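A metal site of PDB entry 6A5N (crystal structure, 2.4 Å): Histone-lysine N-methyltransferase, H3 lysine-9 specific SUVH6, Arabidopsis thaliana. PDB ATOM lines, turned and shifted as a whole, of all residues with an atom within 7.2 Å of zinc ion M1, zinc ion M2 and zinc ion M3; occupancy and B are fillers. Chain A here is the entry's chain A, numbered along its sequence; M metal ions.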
ATOM      1  N   LYS A 288       2.568  14.421  15.993  1.00  0.00           N
ATOM      2  CA  LYS A 288       1.848  15.257  15.040  1.00  0.00           C
ATOM      3  C   LYS A 288       0.625  14.467  14.528  1.00  0.00           C
ATOM      4  O   LYS A 288       0.709  13.255  14.346  1.00  0.00           O
ATOM      5  CB  LYS A 288       2.768  15.682  13.888  1.00  0.00           C
ATOM      6  CG  LYS A 288       2.870  17.208  13.668  1.00  0.00           C
ATOM      7  CD  LYS A 288       3.958  17.836  14.543  1.00  0.00           C
ATOM      8  CE  LYS A 288       4.024  19.358  14.403  1.00  0.00           C
ATOM      9  NZ  LYS A 288       2.699  19.993  14.587  1.00  0.00           N
ATOM     10  N   SER A 289      -0.504  15.161  14.334  1.00  0.00           N
ATOM     11  CA  SER A 289      -1.781  14.542  13.939  1.00  0.00           C
ATOM     12  C   SER A 289      -2.338  15.171  12.658  1.00  0.00           C
ATOM     13  O   SER A 289      -1.871  16.235  12.248  1.00  0.00           O
ATOM     14  CB  SER A 289      -2.808  14.693  15.076  1.00  0.00           C
ATOM     15  OG  SER A 289      -2.280  14.220  16.305  1.00  0.00           O
ATOM     16  N   CYS A 290      -3.322  14.522  12.022  1.00  0.00           N
ATOM     17  CA  CYS A 290      -3.959  15.080  10.821  1.00  0.00           C
ATOM     18  C   CYS A 290      -5.235  15.821  11.171  1.00  0.00           C
ATOM     19  O   CYS A 290      -5.787  15.640  12.254  1.00  0.00           O
ATOM     20  CB  CYS A 290      -4.240  13.978   9.777  1.00  0.00           C
ATOM     21  SG  CYS A 290      -5.613  12.829  10.155  1.00  0.00           S
ATOM     22  N   CYS A 291      -5.733  16.634  10.235  1.00  0.00           N
ATOM     23  CA  CYS A 291      -6.906  17.459  10.469  1.00  0.00           C
ATOM     24  C   CYS A 291      -8.114  17.041   9.624  1.00  0.00           C
ATOM     25  O   CYS A 291      -9.074  17.804   9.510  1.00  0.00           O
ATOM     26  CB  CYS A 291      -6.564  18.931  10.195  1.00  0.00           C
ATOM     27  SG  CYS A 291      -5.132  19.529  11.081  1.00  0.00           S
ATOM     28  N   CYS A 292      -8.072  15.846   9.050  1.00  0.00           N
ATOM     29  CA  CYS A 292      -9.090  15.423   8.100  1.00  0.00           C
ATOM     30  C   CYS A 292     -10.493  15.247   8.722  1.00  0.00           C
ATOM     31  O   CYS A 292     -10.636  14.643   9.794  1.00  0.00           O
ATOM     32  CB  CYS A 292      -8.648  14.138   7.398  1.00  0.00           C
ATOM     33  SG  CYS A 292      -7.111  14.264   6.396  1.00  0.00           S
ATOM     34  N   THR A 293     -11.502  15.791   8.047  1.00  0.00           N
ATOM     35  CA  THR A 293     -12.912  15.674   8.446  1.00  0.00           C
ATOM     36  C   THR A 293     -13.396  14.252   8.166  1.00  0.00           C
ATOM     37  O   THR A 293     -14.003  13.606   9.025  1.00  0.00           O
ATOM     38  CB  THR A 293     -13.838  16.648   7.676  1.00  0.00           C
ATOM     39  OG1 THR A 293     -13.911  16.260   6.299  1.00  0.00           O
ATOM     40  CG2 THR A 293     -13.341  18.088   7.775  1.00  0.00           C
ATOM     41  N   THR A 294     -13.134  13.805   6.947  1.00  0.00           N
ATOM     42  CA  THR A 294     -13.511  12.479   6.470  1.00  0.00           C
ATOM     43  C   THR A 294     -12.387  11.450   6.706  1.00  0.00           C
ATOM     44  O   THR A 294     -11.431  11.740   7.430  1.00  0.00           O
ATOM     45  CB  THR A 294     -13.871  12.520   4.976  1.00  0.00           C
ATOM     46  OG1 THR A 294     -14.261  11.207   4.523  1.00  0.00           O
ATOM     47  CG2 THR A 294     -12.681  13.008   4.158  1.00  0.00           C
ATOM     48  N   ARG A 295     -12.515  10.263   6.115  1.00  0.00           N
ATOM     49  CA  ARG A 295     -11.490   9.218   6.217  1.00  0.00           C
ATOM     50  C   ARG A 295     -10.233   9.585   5.452  1.00  0.00           C
ATOM     51  O   ARG A 295     -10.296  10.152   4.358  1.00  0.00           O
ATOM     52  CB  ARG A 295     -12.025   7.882   5.718  1.00  0.00           C
ATOM     53  CG  ARG A 295     -13.110   7.287   6.586  1.00  0.00           C
ATOM     54  CD  ARG A 295     -13.511   5.916   6.075  1.00  0.00           C
ATOM     55  NE  ARG A 295     -14.175   6.037   4.784  1.00  0.00           N
ATOM     56  CZ  ARG A 295     -15.212   5.291   4.409  1.00  0.00           C
ATOM     57  NH1 ARG A 295     -15.758   5.472   3.213  1.00  0.00           N
ATOM     58  NH2 ARG A 295     -15.693   4.378   5.222  1.00  0.00           N
ATOM     59  N   CYS A 296      -9.071   9.242   6.014  1.00  0.00           N
ATOM     60  CA  CYS A 296      -7.811   9.657   5.418  1.00  0.00           C
ATOM     61  C   CYS A 296      -7.446   8.770   4.251  1.00  0.00           C
ATOM     62  O   CYS A 296      -7.216   7.557   4.399  1.00  0.00           O
ATOM     63  CB  CYS A 296      -6.704   9.648   6.463  1.00  0.00           C
ATOM     64  SG  CYS A 296      -7.090  10.676   7.875  1.00  0.00           S
ATOM     65  N   THR A 297      -7.424   9.370   3.067  1.00  0.00           N
ATOM     66  CA  THR A 297      -7.069   8.639   1.858  1.00  0.00           C
ATOM     67  C   THR A 297      -6.190   9.520   1.005  1.00  0.00           C
ATOM     68  O   THR A 297      -6.193  10.744   1.174  1.00  0.00           O
ATOM     69  CB  THR A 297      -8.309   8.219   1.042  1.00  0.00           C
ATOM     70  OG1 THR A 297      -8.743   9.333   0.253  1.00  0.00           O
ATOM     71  CG2 THR A 297      -9.427   7.748   1.941  1.00  0.00           C
ATOM     72  N   ARG A 302      -7.725  17.455  -0.115  1.00  0.00           N
ATOM     73  CA  ARG A 302      -6.890  17.879   0.992  1.00  0.00           C
ATOM     74  C   ARG A 302      -5.895  16.807   1.376  1.00  0.00           C
ATOM     75  O   ARG A 302      -6.239  15.630   1.481  1.00  0.00           O
ATOM     76  CB  ARG A 302      -7.732  18.265   2.214  1.00  0.00           C
ATOM     77  CG  ARG A 302      -8.642  19.482   2.019  1.00  0.00           C
ATOM     78  CD  ARG A 302      -9.547  19.651   3.252  1.00  0.00           C
ATOM     79  NE  ARG A 302      -8.903  19.041   4.418  1.00  0.00           N
ATOM     80  CZ  ARG A 302      -9.224  19.315   5.679  1.00  0.00           C
ATOM     81  NH1 ARG A 302     -10.203  20.168   5.963  1.00  0.00           N
ATOM     82  NH2 ARG A 302      -8.566  18.714   6.662  1.00  0.00           N
ATOM     83  N   VAL A 303      -4.647  17.228   1.570  1.00  0.00           N
ATOM     84  CA  VAL A 303      -3.580  16.339   1.998  1.00  0.00           C
ATOM     85  C   VAL A 303      -3.682  16.053   3.492  1.00  0.00           C
ATOM     86  O   VAL A 303      -4.115  16.914   4.265  1.00  0.00           O
ATOM     87  CB  VAL A 303      -2.205  16.950   1.649  1.00  0.00           C
ATOM     88  CG1 VAL A 303      -2.082  18.368   2.189  1.00  0.00           C
ATOM     89  CG2 VAL A 303      -1.076  16.087   2.160  1.00  0.00           C
ATOM     90  N   CYS A 304      -3.309  14.834   3.874  1.00  0.00           N
ATOM     91  CA  CYS A 304      -3.346  14.346   5.255  1.00  0.00           C
ATOM     92  C   CYS A 304      -1.954  14.152   5.818  1.00  0.00           C
ATOM     93  O   CYS A 304      -1.145  13.436   5.230  1.00  0.00           O
ATOM     94  CB  CYS A 304      -4.096  13.011   5.326  1.00  0.00           C
ATOM     95  SG  CYS A 304      -3.651  11.993   6.774  1.00  0.00           S
ATOM     96  N   ALA A 305      -1.671  14.758   6.965  1.00  0.00           N
ATOM     97  CA  ALA A 305      -0.332  14.686   7.558  1.00  0.00           C
ATOM     98  C   ALA A 305       0.159  13.252   7.816  1.00  0.00           C
ATOM     99  O   ALA A 305       1.365  12.980   7.745  1.00  0.00           O
ATOM    100  CB  ALA A 305      -0.306  15.480   8.836  1.00  0.00           C
ATOM    101  N   CYS A 306      -0.766  12.332   8.136  1.00  0.00           N
ATOM    102  CA  CYS A 306      -0.375  10.967   8.449  1.00  0.00           C
ATOM    103  C   CYS A 306      -0.089  10.163   7.175  1.00  0.00           C
ATOM    104  O   CYS A 306       0.809   9.304   7.155  1.00  0.00           O
ATOM    105  CB  CYS A 306      -1.451  10.286   9.293  1.00  0.00           C
ATOM    106  SG  CYS A 306      -1.915  11.157  10.835  1.00  0.00           S
ATOM    107  N   VAL A 307      -0.816  10.458   6.105  1.00  0.00           N
ATOM    108  CA  VAL A 307      -0.470   9.966   4.774  1.00  0.00           C
ATOM    109  C   VAL A 307       0.943  10.405   4.380  1.00  0.00           C
ATOM    110  O   VAL A 307       1.799   9.571   4.095  1.00  0.00           O
ATOM    111  CB  VAL A 307      -1.488  10.474   3.726  1.00  0.00           C
ATOM    112  CG1 VAL A 307      -1.002  10.185   2.313  1.00  0.00           C
ATOM    113  CG2 VAL A 307      -2.819   9.806   3.958  1.00  0.00           C
ATOM    114  N   LYS A 309       3.258  11.301   6.279  1.00  0.00           N
ATOM    115  CA  LYS A 309       4.158  10.547   7.150  1.00  0.00           C
ATOM    116  C   LYS A 309       4.438   9.128   6.611  1.00  0.00           C
ATOM    117  O   LYS A 309       5.566   8.654   6.719  1.00  0.00           O
ATOM    118  CB  LYS A 309       3.592  10.461   8.569  1.00  0.00           C
ATOM    119  CG  LYS A 309       4.286  11.372   9.553  1.00  0.00           C
ATOM    120  CD  LYS A 309       3.930  11.044  10.990  1.00  0.00           C
ATOM    121  CE  LYS A 309       2.453  11.244  11.265  1.00  0.00           C
ATOM    122  NZ  LYS A 309       2.097  11.151  12.715  1.00  0.00           N
ATOM    123  N   GLU A 331      -0.155   4.943  11.910  1.00  0.00           N
ATOM    124  CA  GLU A 331      -1.607   5.037  11.970  1.00  0.00           C
ATOM    125  C   GLU A 331      -2.088   6.384  12.582  1.00  0.00           C
ATOM    126  O   GLU A 331      -1.343   7.018  13.336  1.00  0.00           O
ATOM    127  CB  GLU A 331      -2.172   3.845  12.744  1.00  0.00           C
ATOM    128  CG  GLU A 331      -2.425   2.634  11.848  1.00  0.00           C
ATOM    129  CD  GLU A 331      -2.998   1.439  12.590  1.00  0.00           C
ATOM    130  OE1 GLU A 331      -4.022   1.617  13.278  1.00  0.00           O
ATOM    131  OE2 GLU A 331      -2.468   0.313  12.415  1.00  0.00           O
ATOM    132  N   CYS A 332      -3.313   6.798  12.233  1.00  0.00           N
ATOM    133  CA  CYS A 332      -3.889   8.031  12.768  1.00  0.00           C
ATOM    134  C   CYS A 332      -4.038   7.920  14.287  1.00  0.00           C
ATOM    135  O   CYS A 332      -4.538   6.906  14.812  1.00  0.00           O
ATOM    136  CB  CYS A 332      -5.251   8.312  12.126  1.00  0.00           C
ATOM    137  SG  CYS A 332      -5.203   9.126  10.503  1.00  0.00           S
ATOM    138  N   GLY A 333      -3.595   8.951  14.998  1.00  0.00           N
ATOM    139  CA  GLY A 333      -3.625   8.923  16.452  1.00  0.00           C
ATOM    140  C   GLY A 333      -4.930   9.389  17.080  1.00  0.00           C
ATOM    141  O   GLY A 333      -5.888   9.707  16.377  1.00  0.00           O
ATOM    142  N   LEU A 335      -5.425  12.095  18.634  1.00  0.00           N
ATOM    143  CA  LEU A 335      -5.619  13.533  18.435  1.00  0.00           C
ATOM    144  C   LEU A 335      -5.733  13.881  16.936  1.00  0.00           C
ATOM    145  O   LEU A 335      -5.740  15.053  16.561  1.00  0.00           O
ATOM    146  CB  LEU A 335      -4.478  14.314  19.106  1.00  0.00           C
ATOM    147  CG  LEU A 335      -4.469  14.226  20.640  1.00  0.00           C
ATOM    148  CD1 LEU A 335      -3.493  15.205  21.284  1.00  0.00           C
ATOM    149  CD2 LEU A 335      -5.867  14.433  21.191  1.00  0.00           C
ATOM    150  N   CYS A 336      -5.834  12.847  16.097  1.00  0.00           N
ATOM    151  CA  CYS A 336      -6.304  13.000  14.722  1.00  0.00           C
ATOM    152  C   CYS A 336      -7.811  13.192  14.744  1.00  0.00           C
ATOM    153  O   CYS A 336      -8.467  12.720  15.669  1.00  0.00           O
ATOM    154  CB  CYS A 336      -5.907  11.786  13.892  1.00  0.00           C
ATOM    155  SG  CYS A 336      -4.133  11.608  13.650  1.00  0.00           S
ATOM    156  N   LYS A 337      -8.374  13.879  13.748  1.00  0.00           N
ATOM    157  CA  LYS A 337      -9.800  14.280  13.801  1.00  0.00           C
ATOM    158  C   LYS A 337     -10.728  13.418  12.932  1.00  0.00           C
ATOM    159  O   LYS A 337     -11.941  13.665  12.861  1.00  0.00           O
ATOM    160  CB  LYS A 337      -9.921  15.746  13.406  1.00  0.00           C
ATOM    161  CG  LYS A 337      -9.461  16.736  14.471  1.00  0.00           C
ATOM    162  CD  LYS A 337     -10.294  16.599  15.748  1.00  0.00           C
ATOM    163  CE  LYS A 337      -9.536  17.108  16.977  1.00  0.00           C
ATOM    164  NZ  LYS A 337      -9.535  16.144  18.125  1.00  0.00           N
ATOM    165  N   CYS A 338     -10.143  12.423  12.287  1.00  0.00           N
ATOM    166  CA  CYS A 338     -10.800  11.470  11.398  1.00  0.00           C
ATOM    167  C   CYS A 338     -11.666  10.438  12.117  1.00  0.00           C
ATOM    168  O   CYS A 338     -11.316  10.031  13.229  1.00  0.00           O
ATOM    169  CB  CYS A 338      -9.721  10.734  10.602  1.00  0.00           C
ATOM    170  SG  CYS A 338      -8.414  10.103  11.674  1.00  0.00           S
ATOM    171  N   PRO A 339     -12.768   9.993  11.488  1.00  0.00           N
ATOM    172  CA  PRO A 339     -13.632   8.953  12.049  1.00  0.00           C
ATOM    173  C   PRO A 339     -12.887   7.631  12.299  1.00  0.00           C
ATOM    174  O   PRO A 339     -11.898   7.387  11.612  1.00  0.00           O
ATOM    175  CB  PRO A 339     -14.710   8.765  10.973  1.00  0.00           C
ATOM    176  CG  PRO A 339     -14.677   9.989  10.147  1.00  0.00           C
ATOM    177  CD  PRO A 339     -13.234  10.429  10.149  1.00  0.00           C
ATOM    178  N   CYS A 342     -11.673   5.425   9.509  1.00  0.00           N
ATOM    179  CA  CYS A 342     -10.516   5.813   8.703  1.00  0.00           C
ATOM    180  C   CYS A 342      -9.626   4.610   8.370  1.00  0.00           C
ATOM    181  O   CYS A 342      -9.340   3.766   9.224  1.00  0.00           O
ATOM    182  CB  CYS A 342      -9.716   6.883   9.444  1.00  0.00           C
ATOM    183  SG  CYS A 342      -8.078   7.182   8.765  1.00  0.00           S
ATOM    184  N   TYR A 343      -9.200   4.532   7.116  1.00  0.00           N
ATOM    185  CA  TYR A 343      -8.482   3.364   6.628  1.00  0.00           C
ATOM    186  C   TYR A 343      -7.119   3.292   7.306  1.00  0.00           C
ATOM    187  O   TYR A 343      -6.492   2.229   7.361  1.00  0.00           O
ATOM    188  CB  TYR A 343      -8.356   3.402   5.099  1.00  0.00           C
ATOM    189  CG  TYR A 343      -9.672   3.576   4.368  1.00  0.00           C
ATOM    190  CD1 TYR A 343     -10.653   2.609   4.413  1.00  0.00           C
ATOM    191  CD2 TYR A 343      -9.919   4.709   3.616  1.00  0.00           C
ATOM    192  CE1 TYR A 343     -11.851   2.771   3.737  1.00  0.00           C
ATOM    193  CE2 TYR A 343     -11.109   4.881   2.944  1.00  0.00           C
ATOM    194  CZ  TYR A 343     -12.070   3.911   3.009  1.00  0.00           C
ATOM    195  OH  TYR A 343     -13.249   4.088   2.318  1.00  0.00           O
ATOM    196  N   LEU A 344      -6.670   4.439   7.821  1.00  0.00           N
ATOM    197  CA  LEU A 344      -5.391   4.498   8.520  1.00  0.00           C
ATOM    198  C   LEU A 344      -5.580   4.173  10.010  1.00  0.00           C
ATOM    199  O   LEU A 344      -4.701   4.448  10.839  1.00  0.00           O
ATOM    200  CB  LEU A 344      -4.736   5.885   8.334  1.00  0.00           C
ATOM    201  CG  LEU A 344      -4.097   6.020   6.952  1.00  0.00           C
ATOM    202  CD1 LEU A 344      -3.304   7.304   6.776  1.00  0.00           C
ATOM    203  CD2 LEU A 344      -3.212   4.836   6.666  1.00  0.00           C
ATOM    204  N   ARG A 345      -6.722   3.563  10.330  1.00  0.00           N
ATOM    205  CA  ARG A 345      -6.928   2.907  11.613  1.00  0.00           C
ATOM    206  C   ARG A 345      -7.214   1.430  11.422  1.00  0.00           C
ATOM    207  O   ARG A 345      -8.317   1.072  10.973  1.00  0.00           O
ATOM    208  CB  ARG A 345      -8.098   3.545  12.389  1.00  0.00           C
ATOM    209  CG  ARG A 345      -8.094   5.059  12.409  1.00  0.00           C
ATOM    210  CD  ARG A 345      -8.873   5.573  13.607  1.00  0.00           C
ATOM    211  NE  ARG A 345      -8.955   7.027  13.627  1.00  0.00           N
ATOM    212  CZ  ARG A 345      -8.397   7.803  14.555  1.00  0.00           C
ATOM    213  NH1 ARG A 345      -8.541   9.114  14.501  1.00  0.00           N
ATOM    214  NH2 ARG A 345      -7.693   7.260  15.535  1.00  0.00           N
HETATM  215 ZN    ZN M   1      -7.132   9.474   9.704  1.00  0.00          ZN
HETATM  216 ZN    ZN M   2      -4.037  11.354  11.260  1.00  0.00          ZN
HETATM  217 ZN    ZN M   3      -5.683  12.665   7.594  1.00  0.00          ZN
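Within 4 Å of zinc ion M2: Cys 290, Cys 306, Cys 332 and Cys 336.
Zinc ion M2 is bound by the side-chain sulfur (SG) of Cys 306 (2.2 Å), the side-chain sulfur (SG) of Cys 336 (2.4 Å), the side-chain sulfur (SG) of Cys 290 (2.4 Å) and the side-chain sulfur (SG) of Cys 332 (2.6 Å). Zinc ion M2 has four donor atoms within binding distance.
The side-chain sulfur (SG) of Cys 304 sits close to the backbone NH (N) of Val 307, 3.3 Å away. SG of Cys 336 lies close to N of Gly 333, 3.0 Å away. The guanidinium group (NH2) of Arg 345 is in hydrogen-bond range of the backbone carbonyl oxygen (O) of Cys 332, 3.3 Å away. The backbone carbonyl oxygen of Cys 292 sits at hydrogen-bond distance from the backbone NH of Cys 338, at 3.4 Å. N of Leu 344 sits close to SG of Cys 342. SG of Cys 304 lies close to N of Cys 306 (3.2 Å). The backbone carbonyl oxygen of Cys 338 is in hydrogen-bond range of the guanidinium group of Arg 345 (3.2 Å). The backbone carbonyl oxygen of Leu 344 sits at hydrogen-bond distance from the backbone NH of Cys 332, 3.1 Å away.
Zinc ion M3 is bound by SG of Cys 304. The side-chain sulfur (SG) of Cys 296 binds zinc ion M3. Zinc ion M3 is bound by the side-chain sulfur (SG) of Cys 292, at 2.5 Å. SG of Cys 290 binds zinc ion M3 (2.6 Å). Zinc ion M3 has four donor atoms within binding distance.
Zinc ion M1 is bound by SG of Cys 332 (2.1 Å), SG of Cys 296 (2.2 Å), SG of Cys 338 (2.4 Å) and SG of Cys 342 (2.7 Å). Zinc ion M1 has four donor atoms within binding distance.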
